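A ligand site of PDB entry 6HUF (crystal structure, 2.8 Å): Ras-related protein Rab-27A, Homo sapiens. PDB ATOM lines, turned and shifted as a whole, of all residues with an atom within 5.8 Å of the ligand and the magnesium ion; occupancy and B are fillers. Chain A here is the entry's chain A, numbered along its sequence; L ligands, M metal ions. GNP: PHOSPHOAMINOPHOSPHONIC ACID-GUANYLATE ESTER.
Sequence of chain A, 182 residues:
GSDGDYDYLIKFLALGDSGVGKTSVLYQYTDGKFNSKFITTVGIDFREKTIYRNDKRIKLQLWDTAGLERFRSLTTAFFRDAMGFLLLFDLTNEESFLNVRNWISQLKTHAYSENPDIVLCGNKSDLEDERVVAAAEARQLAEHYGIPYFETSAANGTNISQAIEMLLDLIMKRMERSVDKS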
ATOM      1  N   GLY A  16      26.106 -13.901  13.939  1.00  0.00           N
ATOM      2  CA  GLY A  16      24.780 -14.195  13.350  1.00  0.00           C
ATOM      3  C   GLY A  16      24.757 -15.619  12.849  1.00  0.00           C
ATOM      4  O   GLY A  16      25.678 -16.376  13.202  1.00  0.00           O
ATOM      5  N   ASP A  17      23.768 -15.954  12.018  1.00  0.00           N
ATOM      6  CA  ASP A  17      23.521 -17.337  11.561  1.00  0.00           C
ATOM      7  C   ASP A  17      24.316 -17.594  10.280  1.00  0.00           C
ATOM      8  O   ASP A  17      24.832 -16.642   9.710  1.00  0.00           O
ATOM      9  CB  ASP A  17      22.024 -17.597  11.416  1.00  0.00           C
ATOM     10  CG  ASP A  17      21.277 -17.564  12.744  1.00  0.00           C
ATOM     11  OD1 ASP A  17      21.926 -17.243  13.783  1.00  0.00           O
ATOM     12  OD2 ASP A  17      20.073 -17.872  12.738  1.00  0.00           O
ATOM     13  N   SER A  18      24.437 -18.854   9.893  1.00  0.00           N
ATOM     14  CA  SER A  18      25.048 -19.310   8.637  1.00  0.00           C
ATOM     15  C   SER A  18      24.170 -18.848   7.465  1.00  0.00           C
ATOM     16  O   SER A  18      22.970 -19.195   7.447  1.00  0.00           O
ATOM     17  CB  SER A  18      25.239 -20.817   8.657  1.00  0.00           C
ATOM     18  OG  SER A  18      26.029 -21.260   7.562  1.00  0.00           O
ATOM     19  N   GLY A  19      24.748 -18.061   6.539  1.00  0.00           N
ATOM     20  CA  GLY A  19      24.111 -17.650   5.273  1.00  0.00           C
ATOM     21  C   GLY A  19      23.748 -16.168   5.278  1.00  0.00           C
ATOM     22  O   GLY A  19      23.398 -15.619   4.200  1.00  0.00           O
ATOM     23  N   VAL A  20      23.812 -15.543   6.454  1.00  0.00           N
ATOM     24  CA  VAL A  20      23.481 -14.114   6.672  1.00  0.00           C
ATOM     25  C   VAL A  20      24.267 -13.271   5.656  1.00  0.00           C
ATOM     26  O   VAL A  20      23.629 -12.564   4.860  1.00  0.00           O
ATOM     27  CB  VAL A  20      23.798 -13.708   8.122  1.00  0.00           C
ATOM     28  CG1 VAL A  20      23.930 -12.208   8.265  1.00  0.00           C
ATOM     29  CG2 VAL A  20      22.766 -14.231   9.100  1.00  0.00           C
ATOM     30  N   GLY A  21      25.595 -13.389   5.692  1.00  0.00           N
ATOM     31  CA  GLY A  21      26.522 -12.737   4.752  1.00  0.00           C
ATOM     32  C   GLY A  21      27.572 -11.905   5.452  1.00  0.00           C
ATOM     33  O   GLY A  21      27.978 -10.886   4.873  1.00  0.00           O
ATOM     34  N   LYS A  22      28.039 -12.336   6.628  1.00  0.00           N
ATOM     35  CA  LYS A  22      28.955 -11.534   7.491  1.00  0.00           C
ATOM     36  C   LYS A  22      30.392 -11.629   6.954  1.00  0.00           C
ATOM     37  O   LYS A  22      31.203 -10.753   7.322  1.00  0.00           O
ATOM     38  CB  LYS A  22      28.883 -11.991   8.952  1.00  0.00           C
ATOM     39  CG  LYS A  22      28.636 -13.471   9.149  1.00  0.00           C
ATOM     40  CD  LYS A  22      28.638 -13.919  10.573  1.00  0.00           C
ATOM     41  CE  LYS A  22      28.337 -15.395  10.647  1.00  0.00           C
ATOM     42  NZ  LYS A  22      27.721 -15.744  11.940  1.00  0.00           N
ATOM     43  N   THR A  23      30.695 -12.627   6.123  1.00  0.00           N
ATOM     44  CA  THR A  23      31.994 -12.749   5.421  1.00  0.00           C
ATOM     45  C   THR A  23      31.972 -11.791   4.220  1.00  0.00           C
ATOM     46  O   THR A  23      32.965 -11.069   4.025  1.00  0.00           O
ATOM     47  CB  THR A  23      32.271 -14.188   5.002  1.00  0.00           C
ATOM     48  OG1 THR A  23      31.969 -15.058   6.093  1.00  0.00           O
ATOM     49  CG2 THR A  23      33.713 -14.405   4.592  1.00  0.00           C
ATOM     50  N   SER A  24      30.871 -11.799   3.469  1.00  0.00           N
ATOM     51  CA  SER A  24      30.682 -10.962   2.256  1.00  0.00           C
ATOM     52  C   SER A  24      30.646  -9.492   2.677  1.00  0.00           C
ATOM     53  O   SER A  24      31.166  -8.641   1.910  1.00  0.00           O
ATOM     54  CB  SER A  24      29.455 -11.394   1.491  1.00  0.00           C
ATOM     55  OG  SER A  24      29.449 -12.804   1.286  1.00  0.00           O
ATOM     56  N   VAL A  25      30.110  -9.208   3.870  1.00  0.00           N
ATOM     57  CA  VAL A  25      29.893  -7.836   4.417  1.00  0.00           C
ATOM     58  C   VAL A  25      31.229  -7.248   4.846  1.00  0.00           C
ATOM     59  O   VAL A  25      31.460  -6.074   4.551  1.00  0.00           O
ATOM     60  CB  VAL A  25      28.870  -7.820   5.564  1.00  0.00           C
ATOM     61  CG1 VAL A  25      28.994  -6.591   6.457  1.00  0.00           C
ATOM     62  CG2 VAL A  25      27.435  -7.936   5.027  1.00  0.00           C
ATOM     63  N   PHE A  34      32.640  -7.096  -3.913  1.00  0.00           N
ATOM     64  CA  PHE A  34      31.784  -8.232  -3.519  1.00  0.00           C
ATOM     65  C   PHE A  34      32.318  -9.524  -4.144  1.00  0.00           C
ATOM     66  O   PHE A  34      32.221  -9.643  -5.383  1.00  0.00           O
ATOM     67  CB  PHE A  34      30.351  -7.936  -3.961  1.00  0.00           C
ATOM     68  CG  PHE A  34      29.344  -9.029  -3.720  1.00  0.00           C
ATOM     69  CD1 PHE A  34      29.158  -9.532  -2.446  1.00  0.00           C
ATOM     70  CD2 PHE A  34      28.607  -9.565  -4.761  1.00  0.00           C
ATOM     71  CE1 PHE A  34      28.247 -10.553  -2.210  1.00  0.00           C
ATOM     72  CE2 PHE A  34      27.716 -10.610  -4.526  1.00  0.00           C
ATOM     73  CZ  PHE A  34      27.542 -11.094  -3.249  1.00  0.00           C
ATOM     74  N   ASN A  35      32.889 -10.416  -3.315  1.00  0.00           N
ATOM     75  CA  ASN A  35      33.150 -11.834  -3.683  1.00  0.00           C
ATOM     76  C   ASN A  35      31.853 -12.586  -3.410  1.00  0.00           C
ATOM     77  O   ASN A  35      31.472 -12.679  -2.236  1.00  0.00           O
ATOM     78  CB  ASN A  35      34.347 -12.455  -2.949  1.00  0.00           C
ATOM     79  N   SER A  36      31.201 -13.092  -4.453  1.00  0.00           N
ATOM     80  CA  SER A  36      30.002 -13.957  -4.329  1.00  0.00           C
ATOM     81  C   SER A  36      30.432 -15.359  -3.863  1.00  0.00           C
ATOM     82  O   SER A  36      29.585 -16.043  -3.280  1.00  0.00           O
ATOM     83  CB  SER A  36      29.206 -13.976  -5.614  1.00  0.00           C
ATOM     84  OG  SER A  36      29.971 -14.422  -6.725  1.00  0.00           O
ATOM     85  N   LYS A  37      31.688 -15.756  -4.105  1.00  0.00           N
ATOM     86  CA  LYS A  37      32.260 -17.040  -3.643  1.00  0.00           C
ATOM     87  C   LYS A  37      32.631 -16.910  -2.151  1.00  0.00           C
ATOM     88  O   LYS A  37      33.238 -15.908  -1.765  1.00  0.00           O
ATOM     89  CB  LYS A  37      33.442 -17.449  -4.518  1.00  0.00           C
ATOM     90  N   PHE A  38      32.166 -17.825  -1.318  1.00  0.00           N
ATOM     91  CA  PHE A  38      32.512 -17.855   0.119  1.00  0.00           C
ATOM     92  C   PHE A  38      32.169 -19.241   0.640  1.00  0.00           C
ATOM     93  O   PHE A  38      30.999 -19.625   0.627  1.00  0.00           O
ATOM     94  CB  PHE A  38      31.837 -16.710   0.878  1.00  0.00           C
ATOM     95  N   ILE A  39      33.202 -20.011   0.984  1.00  0.00           N
ATOM     96  CA  ILE A  39      33.058 -21.286   1.719  1.00  0.00           C
ATOM     97  C   ILE A  39      32.306 -20.925   3.016  1.00  0.00           C
ATOM     98  O   ILE A  39      32.595 -19.853   3.594  1.00  0.00           O
ATOM     99  CB  ILE A  39      34.440 -21.939   1.943  1.00  0.00           C
ATOM    100  N   THR A  40      31.329 -21.738   3.418  1.00  0.00           N
ATOM    101  CA  THR A  40      30.676 -21.572   4.747  1.00  0.00           C
ATOM    102  C   THR A  40      31.797 -21.712   5.773  1.00  0.00           C
ATOM    103  O   THR A  40      32.187 -22.840   6.054  1.00  0.00           O
ATOM    104  CB  THR A  40      29.489 -22.527   4.940  1.00  0.00           C
ATOM    105  OG1 THR A  40      29.968 -23.865   4.869  1.00  0.00           O
ATOM    106  CG2 THR A  40      28.392 -22.350   3.918  1.00  0.00           C
ATOM    107  N   THR A  41      32.362 -20.581   6.203  1.00  0.00           N
ATOM    108  CA  THR A  41      33.445 -20.410   7.202  1.00  0.00           C
ATOM    109  C   THR A  41      33.559 -21.564   8.213  1.00  0.00           C
ATOM    110  O   THR A  41      32.550 -21.838   8.900  1.00  0.00           O
ATOM    111  CB  THR A  41      33.201 -19.139   8.026  1.00  0.00           C
ATOM    112  OG1 THR A  41      33.157 -18.032   7.134  1.00  0.00           O
ATOM    113  CG2 THR A  41      34.237 -18.918   9.103  1.00  0.00           C
ATOM    114  N   ASP A  64      35.667 -12.244  11.986  1.00  0.00           N
ATOM    115  CA  ASP A  64      34.588 -13.060  11.371  1.00  0.00           C
ATOM    116  C   ASP A  64      34.462 -14.317  12.245  1.00  0.00           C
ATOM    117  O   ASP A  64      35.462 -14.703  12.876  1.00  0.00           O
ATOM    118  CB  ASP A  64      34.916 -13.369   9.905  1.00  0.00           C
ATOM    119  CG  ASP A  64      33.742 -13.870   9.044  1.00  0.00           C
ATOM    120  OD1 ASP A  64      32.766 -14.410   9.612  1.00  0.00           O
ATOM    121  OD2 ASP A  64      33.859 -13.770   7.810  1.00  0.00           O
ATOM    122  N   THR A  65      33.266 -14.899  12.303  1.00  0.00           N
ATOM    123  CA  THR A  65      32.967 -16.130  13.067  1.00  0.00           C
ATOM    124  C   THR A  65      32.253 -17.133  12.155  1.00  0.00           C
ATOM    125  O   THR A  65      31.738 -16.729  11.080  1.00  0.00           O
ATOM    126  CB  THR A  65      32.126 -15.830  14.318  1.00  0.00           C
ATOM    127  OG1 THR A  65      30.925 -15.135  13.943  1.00  0.00           O
ATOM    128  CG2 THR A  65      32.874 -14.998  15.326  1.00  0.00           C
ATOM    129  N   ALA A  66      32.285 -18.400  12.573  1.00  0.00           N
ATOM    130  CA  ALA A  66      31.534 -19.503  11.941  1.00  0.00           C
ATOM    131  C   ALA A  66      30.072 -19.393  12.382  1.00  0.00           C
ATOM    132  O   ALA A  66      29.815 -19.289  13.619  1.00  0.00           O
ATOM    133  CB  ALA A  66      32.155 -20.816  12.319  1.00  0.00           C
ATOM    134  N   GLY A  67      29.162 -19.395  11.405  1.00  0.00           N
ATOM    135  CA  GLY A  67      27.707 -19.258  11.628  1.00  0.00           C
ATOM    136  C   GLY A  67      27.095 -20.479  12.302  1.00  0.00           C
ATOM    137  O   GLY A  67      25.967 -20.361  12.790  1.00  0.00           O
ATOM    138  N   LEU A  68      27.802 -21.611  12.334  1.00  0.00           N
ATOM    139  CA  LEU A  68      27.237 -22.896  12.809  1.00  0.00           C
ATOM    140  C   LEU A  68      27.541 -23.086  14.288  1.00  0.00           C
ATOM    141  O   LEU A  68      27.621 -24.254  14.699  1.00  0.00           O
ATOM    142  CB  LEU A  68      27.793 -24.035  11.953  1.00  0.00           C
ATOM    143  CG  LEU A  68      27.436 -23.971  10.465  1.00  0.00           C
ATOM    144  CD1 LEU A  68      28.168 -25.033   9.670  1.00  0.00           C
ATOM    145  CD2 LEU A  68      25.935 -24.117  10.276  1.00  0.00           C
ATOM    146  N   ASN A 123      20.813  -7.937   6.250  1.00  0.00           N
ATOM    147  CA  ASN A 123      21.620  -8.006   5.004  1.00  0.00           C
ATOM    148  C   ASN A 123      20.770  -8.532   3.845  1.00  0.00           C
ATOM    149  O   ASN A 123      19.624  -8.913   4.081  1.00  0.00           O
ATOM    150  CB  ASN A 123      22.853  -8.868   5.232  1.00  0.00           C
ATOM    151  CG  ASN A 123      23.970  -8.536   4.268  1.00  0.00           C
ATOM    152  OD1 ASN A 123      24.147  -7.364   3.923  1.00  0.00           O
ATOM    153  ND2 ASN A 123      24.701  -9.548   3.848  1.00  0.00           N
ATOM    154  N   LYS A 124      21.344  -8.552   2.648  1.00  0.00           N
ATOM    155  CA  LYS A 124      20.773  -9.163   1.430  1.00  0.00           C
ATOM    156  C   LYS A 124      19.521  -8.363   1.032  1.00  0.00           C
ATOM    157  O   LYS A 124      18.539  -8.957   0.567  1.00  0.00           O
ATOM    158  CB  LYS A 124      20.542 -10.661   1.694  1.00  0.00           C
ATOM    159  N   SER A 125      19.574  -7.044   1.201  1.00  0.00           N
ATOM    160  CA  SER A 125      18.439  -6.113   0.935  1.00  0.00           C
ATOM    161  C   SER A 125      18.192  -6.028  -0.575  1.00  0.00           C
ATOM    162  O   SER A 125      17.046  -5.746  -0.985  1.00  0.00           O
ATOM    163  CB  SER A 125      18.679  -4.758   1.567  1.00  0.00           C
ATOM    164  OG  SER A 125      19.661  -4.009   0.850  1.00  0.00           O
ATOM    165  N   ASP A 126      19.237  -6.269  -1.383  1.00  0.00           N
ATOM    166  CA  ASP A 126      19.154  -6.303  -2.868  1.00  0.00           C
ATOM    167  C   ASP A 126      18.155  -7.387  -3.307  1.00  0.00           C
ATOM    168  O   ASP A 126      17.464  -7.190  -4.328  1.00  0.00           O
ATOM    169  CB  ASP A 126      20.513  -6.541  -3.508  1.00  0.00           C
ATOM    170  CG  ASP A 126      21.260  -7.745  -2.952  1.00  0.00           C
ATOM    171  OD1 ASP A 126      21.479  -7.784  -1.720  1.00  0.00           O
ATOM    172  OD2 ASP A 126      21.607  -8.650  -3.760  1.00  0.00           O
ATOM    173  N   LEU A 127      18.087  -8.487  -2.566  1.00  0.00           N
ATOM    174  CA  LEU A 127      17.138  -9.604  -2.845  1.00  0.00           C
ATOM    175  C   LEU A 127      15.714  -9.134  -2.511  1.00  0.00           C
ATOM    176  O   LEU A 127      15.069  -9.717  -1.622  1.00  0.00           O
ATOM    177  CB  LEU A 127      17.557 -10.834  -2.034  1.00  0.00           C
ATOM    178  CG  LEU A 127      18.968 -11.354  -2.324  1.00  0.00           C
ATOM    179  CD1 LEU A 127      19.301 -12.543  -1.418  1.00  0.00           C
ATOM    180  CD2 LEU A 127      19.124 -11.744  -3.791  1.00  0.00           C
ATOM    181  N   THR A 152      21.324  -3.555   4.912  1.00  0.00           N
ATOM    182  CA  THR A 152      22.627  -3.604   4.208  1.00  0.00           C
ATOM    183  C   THR A 152      22.503  -4.555   3.004  1.00  0.00           C
ATOM    184  O   THR A 152      21.534  -5.361   2.960  1.00  0.00           O
ATOM    185  CB  THR A 152      23.757  -3.979   5.171  1.00  0.00           C
ATOM    186  OG1 THR A 152      23.543  -5.299   5.689  1.00  0.00           O
ATOM    187  CG2 THR A 152      23.879  -3.017   6.324  1.00  0.00           C
ATOM    188  N   SER A 153      23.441  -4.405   2.080  1.00  0.00           N
ATOM    189  CA  SER A 153      23.748  -5.363   0.982  1.00  0.00           C
ATOM    190  C   SER A 153      25.262  -5.361   0.748  1.00  0.00           C
ATOM    191  O   SER A 153      25.839  -4.291   0.533  1.00  0.00           O
ATOM    192  CB  SER A 153      22.994  -5.032  -0.276  1.00  0.00           C
ATOM    193  OG  SER A 153      23.410  -5.865  -1.348  1.00  0.00           O
ATOM    194  N   ALA A 154      25.875  -6.532   0.825  1.00  0.00           N
ATOM    195  CA  ALA A 154      27.308  -6.736   0.495  1.00  0.00           C
ATOM    196  C   ALA A 154      27.456  -6.752  -1.021  1.00  0.00           C
ATOM    197  O   ALA A 154      28.587  -6.573  -1.497  1.00  0.00           O
ATOM    198  CB  ALA A 154      27.826  -8.004   1.144  1.00  0.00           C
ATOM    199  N   ALA A 155      26.360  -6.963  -1.741  1.00  0.00           N
ATOM    200  CA  ALA A 155      26.323  -6.942  -3.224  1.00  0.00           C
ATOM    201  C   ALA A 155      26.355  -5.501  -3.719  1.00  0.00           C
ATOM    202  O   ALA A 155      27.113  -5.244  -4.645  1.00  0.00           O
ATOM    203  CB  ALA A 155      25.105  -7.697  -3.714  1.00  0.00           C
HETATM  204  PG  GNP L   1      28.814 -18.427   7.749  1.00  0.00           P
HETATM  205  O1G GNP L   1      28.590 -19.934   7.414  1.00  0.00           O
HETATM  206  O2G GNP L   1      28.152 -18.009   9.060  1.00  0.00           O
HETATM  207  O3G GNP L   1      30.308 -18.001   7.800  1.00  0.00           O
HETATM  208  N3B GNP L   1      28.141 -17.548   6.538  1.00  0.00           N
HETATM  209  PB  GNP L   1      28.238 -15.932   6.285  1.00  0.00           P
HETATM  210  O1B GNP L   1      27.210 -15.297   7.169  1.00  0.00           O
HETATM  211  O2B GNP L   1      29.629 -15.362   6.261  1.00  0.00           O
HETATM  212  O3A GNP L   1      27.642 -15.755   4.842  1.00  0.00           O
HETATM  213  PA  GNP L   1      28.479 -15.419   3.524  1.00  0.00           P
HETATM  214  O1A GNP L   1      29.395 -16.594   3.260  1.00  0.00           O
HETATM  215  O2A GNP L   1      29.062 -14.047   3.566  1.00  0.00           O
HETATM  216  O5' GNP L   1      27.228 -15.365   2.539  1.00  0.00           O
HETATM  217  C5' GNP L   1      26.698 -16.658   2.207  1.00  0.00           C
HETATM  218  C4' GNP L   1      26.062 -16.518   0.860  1.00  0.00           C
HETATM  219  O4' GNP L   1      25.318 -15.291   0.936  1.00  0.00           O
HETATM  220  C3' GNP L   1      27.011 -16.358  -0.340  1.00  0.00           C
HETATM  221  O3' GNP L   1      26.465 -16.974  -1.502  1.00  0.00           O
HETATM  222  C2' GNP L   1      27.034 -14.851  -0.572  1.00  0.00           C
HETATM  223  O2' GNP L   1      27.115 -14.434  -1.906  1.00  0.00           O
HETATM  224  C1' GNP L   1      25.618 -14.499  -0.175  1.00  0.00           C
HETATM  225  N9  GNP L   1      25.417 -13.119   0.232  1.00  0.00           N
HETATM  226  C8  GNP L   1      25.919 -12.495   1.342  1.00  0.00           C
HETATM  227  N7  GNP L   1      25.536 -11.251   1.450  1.00  0.00           N
HETATM  228  C5  GNP L   1      24.693 -11.071   0.366  1.00  0.00           C
HETATM  229  C6  GNP L   1      23.966  -9.928  -0.020  1.00  0.00           C
HETATM  230  O6  GNP L   1      23.924  -8.866   0.605  1.00  0.00           O
HETATM  231  N1  GNP L   1      23.218 -10.167  -1.182  1.00  0.00           N
HETATM  232  C2  GNP L   1      23.199 -11.348  -1.887  1.00  0.00           C
HETATM  233  N2  GNP L   1      22.426 -11.422  -2.990  1.00  0.00           N
HETATM  234  N3  GNP L   1      23.882 -12.428  -1.527  1.00  0.00           N
HETATM  235  C4  GNP L   1      24.610 -12.210  -0.397  1.00  0.00           C
HETATM  236 MG    MG M   1      31.396 -16.711   6.868  1.00  0.00          MG
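N of Ala 155 lies close to OG of Ser 153 (3.2 Å). The backbone NH (N) of Lys 124 is in hydrogen-bond range of the backbone carbonyl oxygen (O) of Thr 152 (3.2 Å). NZ of Lys 22 is in hydrogen-bond range of O of Gly 16 (2.5 Å). The side-chain carboxylate (OD1) of Asp 126 sits at hydrogen-bond distance from the side-chain hydroxyl (OG) of Ser 153 (2.7 Å). The backbone carbonyl oxygen (O) of Val 20 is in hydrogen-bond range of the side-chain amide nitrogen (ND2) of Asn 123 (3.4 Å). OD1 of Asn 123 is in hydrogen-bond range of OG1 of Thr 152, at 2.8 Å. The side-chain carboxylate (OD2) of Asp 64 sits close to the side-chain hydroxyl (OG1) of Thr 23 (2.9 Å).
The backbone NH (N) of Gly 19 lies close to a nitrogen (N3B) of the ligand, 3.4 Å away. Asp 17 touches the ligand. Phe 34 touches the ligand (CZ to O2', 3.6 Å). CB of Phe 38 touches O1A of the ligand, at 3.4 Å. CB of Thr 40 touches O1G of the ligand, 3.7 Å away. Thr 65 touches the ligand. CD2 of Leu 127 touches N2 of the ligand, at 3.4 Å. Ser 153 touches the ligand (CA to O6, 3.5 Å). Ala 155 touches the ligand (N to O6, 3.9 Å). 22 residues have an atom within 4 Å of the ligand: Asp 17, Ser 18, Gly 19, Val 20, Gly 21, Lys 22, Thr 23, Ser 24, Phe 34, Ser 36, Phe 38, Thr 40, Thr 41, Thr 65, Gly 67, Asn 123, Lys 124, Asp 126, Leu 127, Ser 153, Ala 154 and Ala 155. The nearest printed residue that does not touch the ligand is Ala 66 (4.1 Å).
The backbone NH (N) of Ala 154 is in hydrogen-bond range of an oxygen (O6) of the ligand (3.0 Å). A nitrogen (N2) of the ligand lies within hydrogen-bond range of the side-chain carboxylate (OD2) of Asp 126, 3.0 Å away. The backbone carbonyl oxygen of Ser 36 is in hydrogen-bond range of an oxygen (O2') of the ligand (3.3 Å). An oxygen (O2A) of the ligand is in hydrogen-bond range of the side-chain hydroxyl (OG) of Ser 24 (2.6 Å). The backbone NH (N) of Ser 24 sits at hydrogen-bond distance from an oxygen (O2A) of the ligand. An oxygen (O2G) of the ligand lies close to the backbone NH (N) of Gly 67 (2.9 Å). The backbone NH of Lys 22 lies close to an oxygen (O1B) of the ligand (3.1 Å). A nitrogen (N7) of the ligand lies within hydrogen-bond range of the side-chain amide nitrogen (ND2) of Asn 123, at 3.1 Å. An oxygen (O6) of the ligand sits close to the backbone NH of Lys 124, at 3.3 Å. O2G of the ligand is in salt-bridge range of NZ of Lys 22, at 3.7 Å. An oxygen (O1B) of the ligand is in hydrogen-bond range of the backbone NH (N) of Val 20 (3.5 Å). N of Gly 21 sits at hydrogen-bond distance from O1B of the ligand (2.9 Å). OG of Ser 18 lies within hydrogen-bond range of O1G of the ligand (2.9 Å). The backbone NH (N) of Thr 23 sits at hydrogen-bond distance from an oxygen (O2A) of the ligand.
Asp 64 touches the magnesium ion (OD1 to MG, 3.8 Å). Of the 32 residues printed, 3 come within 4 Å of the magnesium ion. Along chain A the residues within 4 Å of the magnesium ion span positions 23 to 64.
The magnesium ion is bound by the side-chain hydroxyl (OG1) of Thr 23 (1.9 Å), an oxygen (O3G) of the ligand (1.9 Å), the side-chain hydroxyl (OG1) of Thr 41 (2.2 Å) and an oxygen (O2B) of the ligand (2.3 Å). The magnesium ion has four donor atoms within binding distance.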
